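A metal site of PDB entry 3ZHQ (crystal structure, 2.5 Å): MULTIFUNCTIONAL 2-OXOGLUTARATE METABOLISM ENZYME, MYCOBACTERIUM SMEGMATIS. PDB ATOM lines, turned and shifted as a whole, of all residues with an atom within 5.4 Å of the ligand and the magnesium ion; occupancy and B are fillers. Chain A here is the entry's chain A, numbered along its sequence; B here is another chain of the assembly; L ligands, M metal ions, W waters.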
ATOM      1  N   HIS A 180      10.713 -21.039 -19.467  1.00  0.00           N
ATOM      2  CA  HIS A 180      10.597 -20.954 -18.024  1.00  0.00           C
ATOM      3  C   HIS A 180      10.572 -22.285 -17.236  1.00  0.00           C
ATOM      4  O   HIS A 180      11.055 -22.309 -16.109  1.00  0.00           O
ATOM      5  CB  HIS A 180       9.379 -20.094 -17.607  1.00  0.00           C
ATOM      6  CG  HIS A 180       8.032 -20.488 -18.158  1.00  0.00           C
ATOM      7  ND1 HIS A 180       7.365 -19.663 -19.079  1.00  0.00           N
ATOM      8  CD2 HIS A 180       7.197 -21.499 -17.800  1.00  0.00           C
ATOM      9  CE1 HIS A 180       6.176 -20.222 -19.278  1.00  0.00           C
ATOM     10  NE2 HIS A 180       6.023 -21.324 -18.540  1.00  0.00           N
ATOM     11  N   ARG A 181       9.996 -23.367 -17.804  1.00  0.00           N
ATOM     12  CA  ARG A 181       9.852 -24.672 -17.136  1.00  0.00           C
ATOM     13  C   ARG A 181      11.226 -25.282 -16.713  1.00  0.00           C
ATOM     14  O   ARG A 181      12.021 -25.696 -17.549  1.00  0.00           O
ATOM     15  CB  ARG A 181       9.052 -25.653 -18.018  1.00  0.00           C
ATOM     16  CG  ARG A 181       8.558 -26.864 -17.251  1.00  0.00           C
ATOM     17  CD  ARG A 181       7.616 -27.777 -18.041  1.00  0.00           C
ATOM     18  NE  ARG A 181       6.438 -27.100 -18.602  1.00  0.00           N
ATOM     19  CZ  ARG A 181       5.368 -26.733 -17.906  1.00  0.00           C
ATOM     20  NH1 ARG A 181       5.304 -26.962 -16.594  1.00  0.00           N
ATOM     21  NH2 ARG A 181       4.350 -26.149 -18.508  1.00  0.00           N
ATOM     22  N   SER A 245       9.025 -14.045 -22.824  1.00  0.00           N
ATOM     23  CA  SER A 245       8.039 -15.119 -22.597  1.00  0.00           C
ATOM     24  C   SER A 245       7.743 -15.792 -23.919  1.00  0.00           C
ATOM     25  O   SER A 245       7.370 -16.960 -23.937  1.00  0.00           O
ATOM     26  CB  SER A 245       6.774 -14.581 -21.944  1.00  0.00           C
ATOM     27  OG  SER A 245       6.899 -14.461 -20.533  1.00  0.00           O
ATOM     28  N   HIS A 246       7.983 -15.061 -25.032  1.00  0.00           N
ATOM     29  CA  HIS A 246       7.840 -15.496 -26.424  1.00  0.00           C
ATOM     30  C   HIS A 246       8.649 -16.749 -26.669  1.00  0.00           C
ATOM     31  O   HIS A 246       9.867 -16.688 -26.856  1.00  0.00           O
ATOM     32  CB  HIS A 246       8.265 -14.364 -27.389  1.00  0.00           C
ATOM     33  CG  HIS A 246       7.299 -13.238 -27.401  1.00  0.00           C
ATOM     34  ND1 HIS A 246       6.954 -12.569 -26.260  1.00  0.00           N
ATOM     35  CD2 HIS A 246       6.597 -12.720 -28.435  1.00  0.00           C
ATOM     36  CE1 HIS A 246       6.065 -11.663 -26.616  1.00  0.00           C
ATOM     37  NE2 HIS A 246       5.814 -11.719 -27.919  1.00  0.00           N
ATOM     38  N   LEU A 247       7.965 -17.900 -26.640  1.00  0.00           N
ATOM     39  CA  LEU A 247       8.568 -19.223 -26.801  1.00  0.00           C
ATOM     40  C   LEU A 247       9.295 -19.314 -28.151  1.00  0.00           C
ATOM     41  O   LEU A 247       8.809 -18.767 -29.138  1.00  0.00           O
ATOM     42  CB  LEU A 247       7.517 -20.340 -26.620  1.00  0.00           C
ATOM     43  CG  LEU A 247       6.837 -20.425 -25.198  1.00  0.00           C
ATOM     44  CD1 LEU A 247       5.502 -21.159 -25.246  1.00  0.00           C
ATOM     45  CD2 LEU A 247       7.767 -21.040 -24.150  1.00  0.00           C
ATOM     46  N   GLY A 285       9.993 -26.752 -25.796  1.00  0.00           N
ATOM     47  CA  GLY A 285       8.727 -27.404 -25.472  1.00  0.00           C
ATOM     48  C   GLY A 285       8.230 -28.075 -26.731  1.00  0.00           C
ATOM     49  O   GLY A 285       8.506 -27.603 -27.838  1.00  0.00           O
ATOM     50  N   ASP A 286       7.506 -29.181 -26.591  1.00  0.00           N
ATOM     51  CA  ASP A 286       6.998 -29.948 -27.735  1.00  0.00           C
ATOM     52  C   ASP A 286       6.032 -29.147 -28.615  1.00  0.00           C
ATOM     53  O   ASP A 286       6.131 -29.273 -29.836  1.00  0.00           O
ATOM     54  CB  ASP A 286       6.328 -31.256 -27.261  1.00  0.00           C
ATOM     55  CG  ASP A 286       5.165 -31.080 -26.300  1.00  0.00           C
ATOM     56  OD1 ASP A 286       5.396 -30.591 -25.172  1.00  0.00           O
ATOM     57  OD2 ASP A 286       4.035 -31.444 -26.676  1.00  0.00           O
ATOM     58  N   ALA A 287       5.109 -28.339 -28.056  1.00  0.00           N
ATOM     59  CA  ALA A 287       4.146 -27.589 -28.892  1.00  0.00           C
ATOM     60  C   ALA A 287       4.850 -26.426 -29.604  1.00  0.00           C
ATOM     61  O   ALA A 287       4.626 -26.207 -30.796  1.00  0.00           O
ATOM     62  CB  ALA A 287       2.950 -27.094 -28.068  1.00  0.00           C
ATOM     63  N   ALA A 288       5.728 -25.701 -28.892  1.00  0.00           N
ATOM     64  CA  ALA A 288       6.465 -24.537 -29.413  1.00  0.00           C
ATOM     65  C   ALA A 288       7.475 -24.931 -30.519  1.00  0.00           C
ATOM     66  O   ALA A 288       7.614 -24.200 -31.497  1.00  0.00           O
ATOM     67  CB  ALA A 288       7.173 -23.826 -28.280  1.00  0.00           C
ATOM     68  N   PHE A 289       8.132 -26.114 -30.377  1.00  0.00           N
ATOM     69  CA  PHE A 289       9.111 -26.613 -31.357  1.00  0.00           C
ATOM     70  C   PHE A 289       8.473 -26.917 -32.699  1.00  0.00           C
ATOM     71  O   PHE A 289       9.091 -26.707 -33.753  1.00  0.00           O
ATOM     72  CB  PHE A 289       9.823 -27.878 -30.830  1.00  0.00           C
ATOM     73  CG  PHE A 289      11.158 -28.178 -31.478  1.00  0.00           C
ATOM     74  CD1 PHE A 289      12.248 -27.352 -31.267  1.00  0.00           C
ATOM     75  CD2 PHE A 289      11.326 -29.295 -32.267  1.00  0.00           C
ATOM     76  CE1 PHE A 289      13.482 -27.642 -31.846  1.00  0.00           C
ATOM     77  CE2 PHE A 289      12.569 -29.574 -32.849  1.00  0.00           C
ATOM     78  CZ  PHE A 289      13.639 -28.756 -32.628  1.00  0.00           C
ATOM     79  N   GLN A 292       6.483 -22.922 -33.992  1.00  0.00           N
ATOM     80  CA  GLN A 292       7.150 -21.634 -34.160  1.00  0.00           C
ATOM     81  C   GLN A 292       8.114 -21.686 -35.344  1.00  0.00           C
ATOM     82  O   GLN A 292       9.028 -22.510 -35.356  1.00  0.00           O
ATOM     83  CB  GLN A 292       7.858 -21.204 -32.860  1.00  0.00           C
ATOM     84  CG  GLN A 292       6.905 -20.772 -31.737  1.00  0.00           C
ATOM     85  CD  GLN A 292       6.224 -19.447 -32.067  1.00  0.00           C
ATOM     86  OE1 GLN A 292       6.874 -18.455 -32.383  1.00  0.00           O
ATOM     87  NE2 GLN A 292       4.884 -19.435 -32.058  1.00  0.00           N
ATOM     88  N   VAL A 317      11.691 -30.965 -24.079  1.00  0.00           N
ATOM     89  CA  VAL A 317      10.976 -31.456 -22.907  1.00  0.00           C
ATOM     90  C   VAL A 317       9.559 -31.773 -23.422  1.00  0.00           C
ATOM     91  O   VAL A 317       8.681 -30.893 -23.409  1.00  0.00           O
ATOM     92  CB  VAL A 317      11.027 -30.437 -21.738  1.00  0.00           C
ATOM     93  CG1 VAL A 317      10.189 -30.917 -20.542  1.00  0.00           C
ATOM     94  CG2 VAL A 317      12.495 -30.179 -21.319  1.00  0.00           C
ATOM     95  N   ASN A 318       9.387 -33.003 -23.975  1.00  0.00           N
ATOM     96  CA  ASN A 318       8.127 -33.458 -24.584  1.00  0.00           C
ATOM     97  C   ASN A 318       7.125 -34.031 -23.545  1.00  0.00           C
ATOM     98  O   ASN A 318       6.982 -35.250 -23.407  1.00  0.00           O
ATOM     99  CB  ASN A 318       8.394 -34.462 -25.706  1.00  0.00           C
ATOM    100  CG  ASN A 318       7.182 -34.708 -26.596  1.00  0.00           C
ATOM    101  OD1 ASN A 318       6.061 -34.272 -26.333  1.00  0.00           O
ATOM    102  ND2 ASN A 318       7.383 -35.422 -27.683  1.00  0.00           N
ATOM    103  N   ASN A 319       6.372 -33.154 -22.902  1.00  0.00           N
ATOM    104  CA  ASN A 319       5.416 -33.558 -21.893  1.00  0.00           C
ATOM    105  C   ASN A 319       4.038 -33.888 -22.532  1.00  0.00           C
ATOM    106  O   ASN A 319       3.065 -34.162 -21.803  1.00  0.00           O
ATOM    107  CB  ASN A 319       5.309 -32.515 -20.806  1.00  0.00           C
ATOM    108  CG  ASN A 319       4.998 -31.120 -21.231  1.00  0.00           C
ATOM    109  OD1 ASN A 319       4.577 -30.853 -22.356  1.00  0.00           O
ATOM    110  ND2 ASN A 319       5.222 -30.194 -20.318  1.00  0.00           N
ATOM    111  N   GLN A 320       3.993 -33.901 -23.893  1.00  0.00           N
ATOM    112  CA  GLN A 320       2.873 -34.369 -24.714  1.00  0.00           C
ATOM    113  C   GLN A 320       1.603 -33.556 -24.477  1.00  0.00           C
ATOM    114  O   GLN A 320       0.475 -34.044 -24.635  1.00  0.00           O
ATOM    115  CB  GLN A 320       2.633 -35.885 -24.451  1.00  0.00           C
ATOM    116  CG  GLN A 320       3.927 -36.739 -24.480  1.00  0.00           C
ATOM    117  CD  GLN A 320       3.761 -38.134 -23.944  1.00  0.00           C
ATOM    118  OE1 GLN A 320       2.826 -38.845 -24.297  1.00  0.00           O
ATOM    119  NE2 GLN A 320       4.684 -38.569 -23.099  1.00  0.00           N
ATOM    120  N   ILE A 321       1.796 -32.299 -24.149  1.00  0.00           N
ATOM    121  CA  ILE A 321       0.709 -31.334 -23.900  1.00  0.00           C
ATOM    122  C   ILE A 321       1.260 -29.947 -24.165  1.00  0.00           C
ATOM    123  O   ILE A 321       2.449 -29.713 -23.987  1.00  0.00           O
ATOM    124  CB  ILE A 321       0.078 -31.473 -22.471  1.00  0.00           C
ATOM    125  CG1 ILE A 321      -1.279 -30.708 -22.385  1.00  0.00           C
ATOM    126  CG2 ILE A 321       1.068 -31.118 -21.332  1.00  0.00           C
ATOM    127  CD1 ILE A 321      -2.174 -31.179 -21.354  1.00  0.00           C
ATOM    128  N   GLY A 322       0.381 -29.057 -24.590  1.00  0.00           N
ATOM    129  CA  GLY A 322       0.711 -27.658 -24.834  1.00  0.00           C
ATOM    130  C   GLY A 322      -0.384 -26.812 -24.233  1.00  0.00           C
ATOM    131  O   GLY A 322      -1.368 -26.490 -24.912  1.00  0.00           O
ATOM    132  N   PHE A 323      -0.240 -26.505 -22.927  1.00  0.00           N
ATOM    133  CA  PHE A 323      -1.190 -25.765 -22.089  1.00  0.00           C
ATOM    134  C   PHE A 323      -2.413 -26.668 -21.891  1.00  0.00           C
ATOM    135  O   PHE A 323      -2.382 -27.519 -21.005  1.00  0.00           O
ATOM    136  CB  PHE A 323      -1.501 -24.372 -22.689  1.00  0.00           C
ATOM    137  CG  PHE A 323      -2.001 -23.320 -21.714  1.00  0.00           C
ATOM    138  CD1 PHE A 323      -3.342 -23.294 -21.330  1.00  0.00           C
ATOM    139  CD2 PHE A 323      -1.162 -22.329 -21.240  1.00  0.00           C
ATOM    140  CE1 PHE A 323      -3.799 -22.337 -20.422  1.00  0.00           C
ATOM    141  CE2 PHE A 323      -1.635 -21.356 -20.370  1.00  0.00           C
ATOM    142  CZ  PHE A 323      -2.960 -21.367 -19.955  1.00  0.00           C
ATOM    143  N   ARG A 384       3.612 -33.694 -17.693  1.00  0.00           N
ATOM    144  CA  ARG A 384       3.422 -32.494 -16.900  1.00  0.00           C
ATOM    145  C   ARG A 384       2.552 -32.830 -15.687  1.00  0.00           C
ATOM    146  O   ARG A 384       1.317 -32.847 -15.809  1.00  0.00           O
ATOM    147  CB  ARG A 384       2.812 -31.375 -17.770  1.00  0.00           C
ATOM    148  CG  ARG A 384       3.110 -29.988 -17.210  1.00  0.00           C
ATOM    149  CD  ARG A 384       2.110 -28.996 -17.710  1.00  0.00           C
ATOM    150  NE  ARG A 384       0.725 -29.439 -17.518  1.00  0.00           N
ATOM    151  CZ  ARG A 384      -0.297 -29.069 -18.294  1.00  0.00           C
ATOM    152  NH1 ARG A 384      -0.096 -28.266 -19.323  1.00  0.00           N
ATOM    153  NH2 ARG A 384      -1.508 -29.526 -18.055  1.00  0.00           N
ATOM    154  N   GLN B 542      -4.882 -20.056 -29.460  1.00  0.00           N
ATOM    155  CA  GLN B 542      -4.240 -20.961 -28.508  1.00  0.00           C
ATOM    156  C   GLN B 542      -5.115 -21.188 -27.286  1.00  0.00           C
ATOM    157  O   GLN B 542      -5.466 -20.244 -26.561  1.00  0.00           O
ATOM    158  CB  GLN B 542      -2.869 -20.425 -28.097  1.00  0.00           C
ATOM    159  CG  GLN B 542      -1.807 -20.715 -29.144  1.00  0.00           C
ATOM    160  CD  GLN B 542      -0.727 -19.669 -29.160  1.00  0.00           C
ATOM    161  OE1 GLN B 542      -0.408 -19.059 -28.148  1.00  0.00           O
ATOM    162  NE2 GLN B 542      -0.136 -19.413 -30.317  1.00  0.00           N
ATOM    163  N   ASP B 543      -5.534 -22.457 -27.080  1.00  0.00           N
ATOM    164  CA  ASP B 543      -6.366 -22.929 -25.972  1.00  0.00           C
ATOM    165  C   ASP B 543      -7.714 -22.201 -25.916  1.00  0.00           C
ATOM    166  O   ASP B 543      -8.275 -22.031 -24.831  1.00  0.00           O
ATOM    167  CB  ASP B 543      -5.609 -22.788 -24.645  1.00  0.00           C
ATOM    168  CG  ASP B 543      -4.265 -23.471 -24.712  1.00  0.00           C
ATOM    169  OD1 ASP B 543      -4.241 -24.727 -24.723  1.00  0.00           O
ATOM    170  OD2 ASP B 543      -3.236 -22.758 -24.846  1.00  0.00           O
ATOM    171  N   LEU B 591       0.767 -23.804 -31.872  1.00  0.00           N
ATOM    172  CA  LEU B 591       1.520 -22.744 -31.199  1.00  0.00           C
ATOM    173  C   LEU B 591       2.191 -21.842 -32.264  1.00  0.00           C
ATOM    174  O   LEU B 591       3.422 -21.744 -32.327  1.00  0.00           O
ATOM    175  CB  LEU B 591       2.542 -23.380 -30.262  1.00  0.00           C
ATOM    176  CG  LEU B 591       3.213 -22.624 -29.110  1.00  0.00           C
ATOM    177  CD1 LEU B 591       3.073 -21.081 -29.148  1.00  0.00           C
ATOM    178  CD2 LEU B 591       2.916 -23.268 -27.812  1.00  0.00           C
ATOM    179  N   GLU B 593       1.591 -17.869 -34.438  1.00  0.00           N
ATOM    180  CA  GLU B 593       0.933 -16.569 -34.520  1.00  0.00           C
ATOM    181  C   GLU B 593       0.874 -16.181 -35.983  1.00  0.00           C
ATOM    182  O   GLU B 593      -0.203 -15.993 -36.519  1.00  0.00           O
ATOM    183  CB  GLU B 593       1.599 -15.494 -33.642  1.00  0.00           C
ATOM    184  CG  GLU B 593       1.290 -15.631 -32.168  1.00  0.00           C
ATOM    185  CD  GLU B 593       2.123 -16.637 -31.384  1.00  0.00           C
ATOM    186  OE1 GLU B 593       3.308 -16.850 -31.742  1.00  0.00           O
ATOM    187  OE2 GLU B 593       1.616 -17.143 -30.368  1.00  0.00           O
ATOM    188  N   GLN B 617      -3.207 -15.671 -27.064  1.00  0.00           N
ATOM    189  CA  GLN B 617      -3.122 -16.209 -25.693  1.00  0.00           C
ATOM    190  C   GLN B 617      -3.163 -14.991 -24.774  1.00  0.00           C
ATOM    191  O   GLN B 617      -4.017 -14.871 -23.897  1.00  0.00           O
ATOM    192  CB  GLN B 617      -1.845 -17.056 -25.520  1.00  0.00           C
ATOM    193  CG  GLN B 617      -1.687 -17.642 -24.128  1.00  0.00           C
ATOM    194  CD  GLN B 617      -2.009 -19.090 -24.070  1.00  0.00           C
ATOM    195  OE1 GLN B 617      -3.099 -19.534 -24.427  1.00  0.00           O
ATOM    196  NE2 GLN B 617      -1.083 -19.858 -23.570  1.00  0.00           N
ATOM    197  N   PHE B 621       1.659 -11.507 -27.660  1.00  0.00           N
ATOM    198  CA  PHE B 621       2.276 -12.466 -28.571  1.00  0.00           C
ATOM    199  C   PHE B 621       1.879 -12.240 -30.044  1.00  0.00           C
ATOM    200  O   PHE B 621       2.512 -12.842 -30.915  1.00  0.00           O
ATOM    201  CB  PHE B 621       1.929 -13.895 -28.124  1.00  0.00           C
ATOM    202  CG  PHE B 621       2.426 -14.174 -26.734  1.00  0.00           C
ATOM    203  CD1 PHE B 621       3.779 -14.067 -26.433  1.00  0.00           C
ATOM    204  CD2 PHE B 621       1.548 -14.517 -25.724  1.00  0.00           C
ATOM    205  CE1 PHE B 621       4.246 -14.303 -25.137  1.00  0.00           C
ATOM    206  CE2 PHE B 621       2.011 -14.739 -24.426  1.00  0.00           C
ATOM    207  CZ  PHE B 621       3.356 -14.632 -24.140  1.00  0.00           C
HETATM  208  N1  LIG L   1       3.219 -17.758 -28.114  1.00  0.00           N
HETATM  209  C1  LIG L   1       4.499 -17.534 -27.846  1.00  0.00           C
HETATM  210  C2  LIG L   1       5.457 -17.225 -28.955  1.00  0.00           C
HETATM  211  N2  LIG L   1       4.980 -17.649 -26.622  1.00  0.00           N
HETATM  212  C3  LIG L   1       4.174 -17.901 -25.570  1.00  0.00           C
HETATM  213  N3  LIG L   1       4.695 -17.861 -24.300  1.00  0.00           N
HETATM  214  C4  LIG L   1       2.800 -18.160 -25.803  1.00  0.00           C
HETATM  215  C5  LIG L   1       2.362 -18.061 -27.127  1.00  0.00           C
HETATM  216  C6  LIG L   1       1.805 -18.509 -24.702  1.00  0.00           C
HETATM  217  N4  LIG L   1       2.059 -19.869 -24.132  1.00  0.00           N
HETATM  218  C7  LIG L   1       2.611 -19.976 -22.962  1.00  0.00           C
HETATM  219  S1  LIG L   1       2.834 -21.614 -22.494  1.00  0.00           S
HETATM  220  C8  LIG L   1       2.073 -22.171 -23.988  1.00  0.00           C
HETATM  221  C9  LIG L   1       1.770 -21.048 -24.716  1.00  0.00           C
HETATM  222  C10 LIG L   1       1.037 -21.242 -26.035  1.00  0.00           C
HETATM  223  C11 LIG L   1       1.917 -23.628 -24.350  1.00  0.00           C
HETATM  224  C12 LIG L   1       3.331 -24.194 -24.263  1.00  0.00           C
HETATM  225  O1  LIG L   1       3.480 -25.461 -24.900  1.00  0.00           O
HETATM  226  P1  LIG L   1       4.893 -26.280 -24.918  1.00  0.00           P
HETATM  227  O2  LIG L   1       5.820 -25.740 -25.945  1.00  0.00           O
HETATM  228  O3  LIG L   1       4.580 -27.802 -25.226  1.00  0.00           O
HETATM  229  O4  LIG L   1       5.585 -26.148 -23.475  1.00  0.00           O
HETATM  230  P2  LIG L   1       5.245 -26.675 -22.104  1.00  0.00           P
HETATM  231  O5  LIG L   1       4.512 -25.525 -21.296  1.00  0.00           O
HETATM  232  O6  LIG L   1       4.395 -27.878 -22.302  1.00  0.00           O
HETATM  233  O7  LIG L   1       6.620 -27.077 -21.383  1.00  0.00           O
HETATM  234 MG    MG M   1       4.491 -29.505 -23.832  1.00  0.00          MG
HETATM  235  O   HOH W   1       1.945 -24.666 -20.483  1.00  0.00           O
HETATM  236  O   HOH W   2       6.817 -29.354 -23.426  1.00  0.00           O
HETATM  237  O   HOH W   3       8.551 -25.724 -22.142  1.00  0.00           O
HETATM  238  O   HOH W   4       1.771 -27.282 -21.171  1.00  0.00           O
HETATM  239  O   HOH W   5       7.859 -24.413 -24.884  1.00  0.00           O
HETATM  240  O   HOH W   6       3.359 -17.147 -21.516  1.00  0.00           O
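Three residues have an atom within 4 Å of the magnesium ion: Asp 286, Asn 319 and Ile 321.
An oxygen (O7) of the ligand is in salt-bridge range of the guanidinium group (NE) of Arg 181 (2.8 Å).
The side-chain carboxylate of Glu 593 of chain B is in hydrogen-bond range of a nitrogen (N1) of the ligand (2.8 Å).
The backbone carbonyl oxygen of Ser 245 is in hydrogen-bond range of a nitrogen (N3) of the ligand.
The backbone NH (N) of Ala 287 lies within hydrogen-bond range of an oxygen (O2) of the ligand (3.4 Å).
An oxygen (O2) of the ligand is in hydrogen-bond range of the backbone NH (N) of Ala 288, at 2.9 Å.
The backbone NH (N) of Leu 247 lies within hydrogen-bond range of a nitrogen (N2) of the ligand, 3.0 Å away.
N4 of the ligand lies close to NE2 of Gln 617 of chain B.
His 246 touches the ligand.
Gly 285 touches the ligand (CA to O2, 3.4 Å).
NE2 of Gln 292 touches C2 of the ligand, 3.9 Å away.
CA of Gly 322 touches O1 of the ligand, 3.5 Å away.
Phe 323 touches the ligand (N to C11, 3.9 Å).
Gln 542 of chain B touches the ligand (OE1 to C5, 3.1 Å).
Leu 591 of chain B touches the ligand (CD2 to C10, 3.3 Å).
Phe 621 of chain B touches the ligand (CZ to N3, 3.5 Å).
Hydrophobic or aromatic side chains that line the ligand: Leu 247, Ala 287, Ala 288, Phe 323, Leu 591 of chain B and Phe 621 of chain B.
Of the 25 residues printed, 18 come within 4 Å of the ligand.
The nearest printed residue that does not touch the ligand is Asp 543 of chain B (4.7 Å).
The magnesium ion is bound by OD1 of Asp 286, OD1 of Asn 319, O of Ile 321, O3 of the ligand, O6 of the ligand and water W2.
OD2 of Asp 286 lies close to OD1 of Asn 318 (3.5 Å).
The side-chain amide nitrogen (NE2) of Gln 542 of chain B is in hydrogen-bond range of the side-chain carboxylate (OE2) of Glu 593 of chain B (2.9 Å).
OE1 of Glu 593 of chain B sits at hydrogen-bond distance from NE2 of Gln 292 (3.0 Å).
O of Gln 542 of chain B lies close to OE1 of Gln 617 of chain B.
The side-chain amide oxygen of Gln 617 of chain B sits close to the side-chain carboxylate of Asp 543 of chain B, 3.3 Å away.
NE2 of Gln 292 sits at hydrogen-bond distance from O of Leu 591 of chain B (2.7 Å).
O of Phe 323 lies within hydrogen-bond range of NH1 of Arg 384 (2.9 Å).
Water W2 lies within hydrogen-bond range of the backbone carbonyl oxygen (O) of Val 317 (2.4 Å), an oxygen (O7) of the ligand (3.1 Å) and the backbone NH (N) of Asp 286 (3.2 Å).
Water W5 bridges O2 of the ligand (2.7 Å) and N of Gly 285 (3.3 Å).
Water W1 lies within hydrogen-bond range of an oxygen (O5) of the ligand and the guanidinium group (NH2) of Arg 181.
Water W4 lies within hydrogen-bond range of the backbone NH (N) of Phe 323 (2.8 Å), the guanidinium group (NH1) of Arg 384 (2.8 Å) and an oxygen (O5) of the ligand (3.3 Å).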
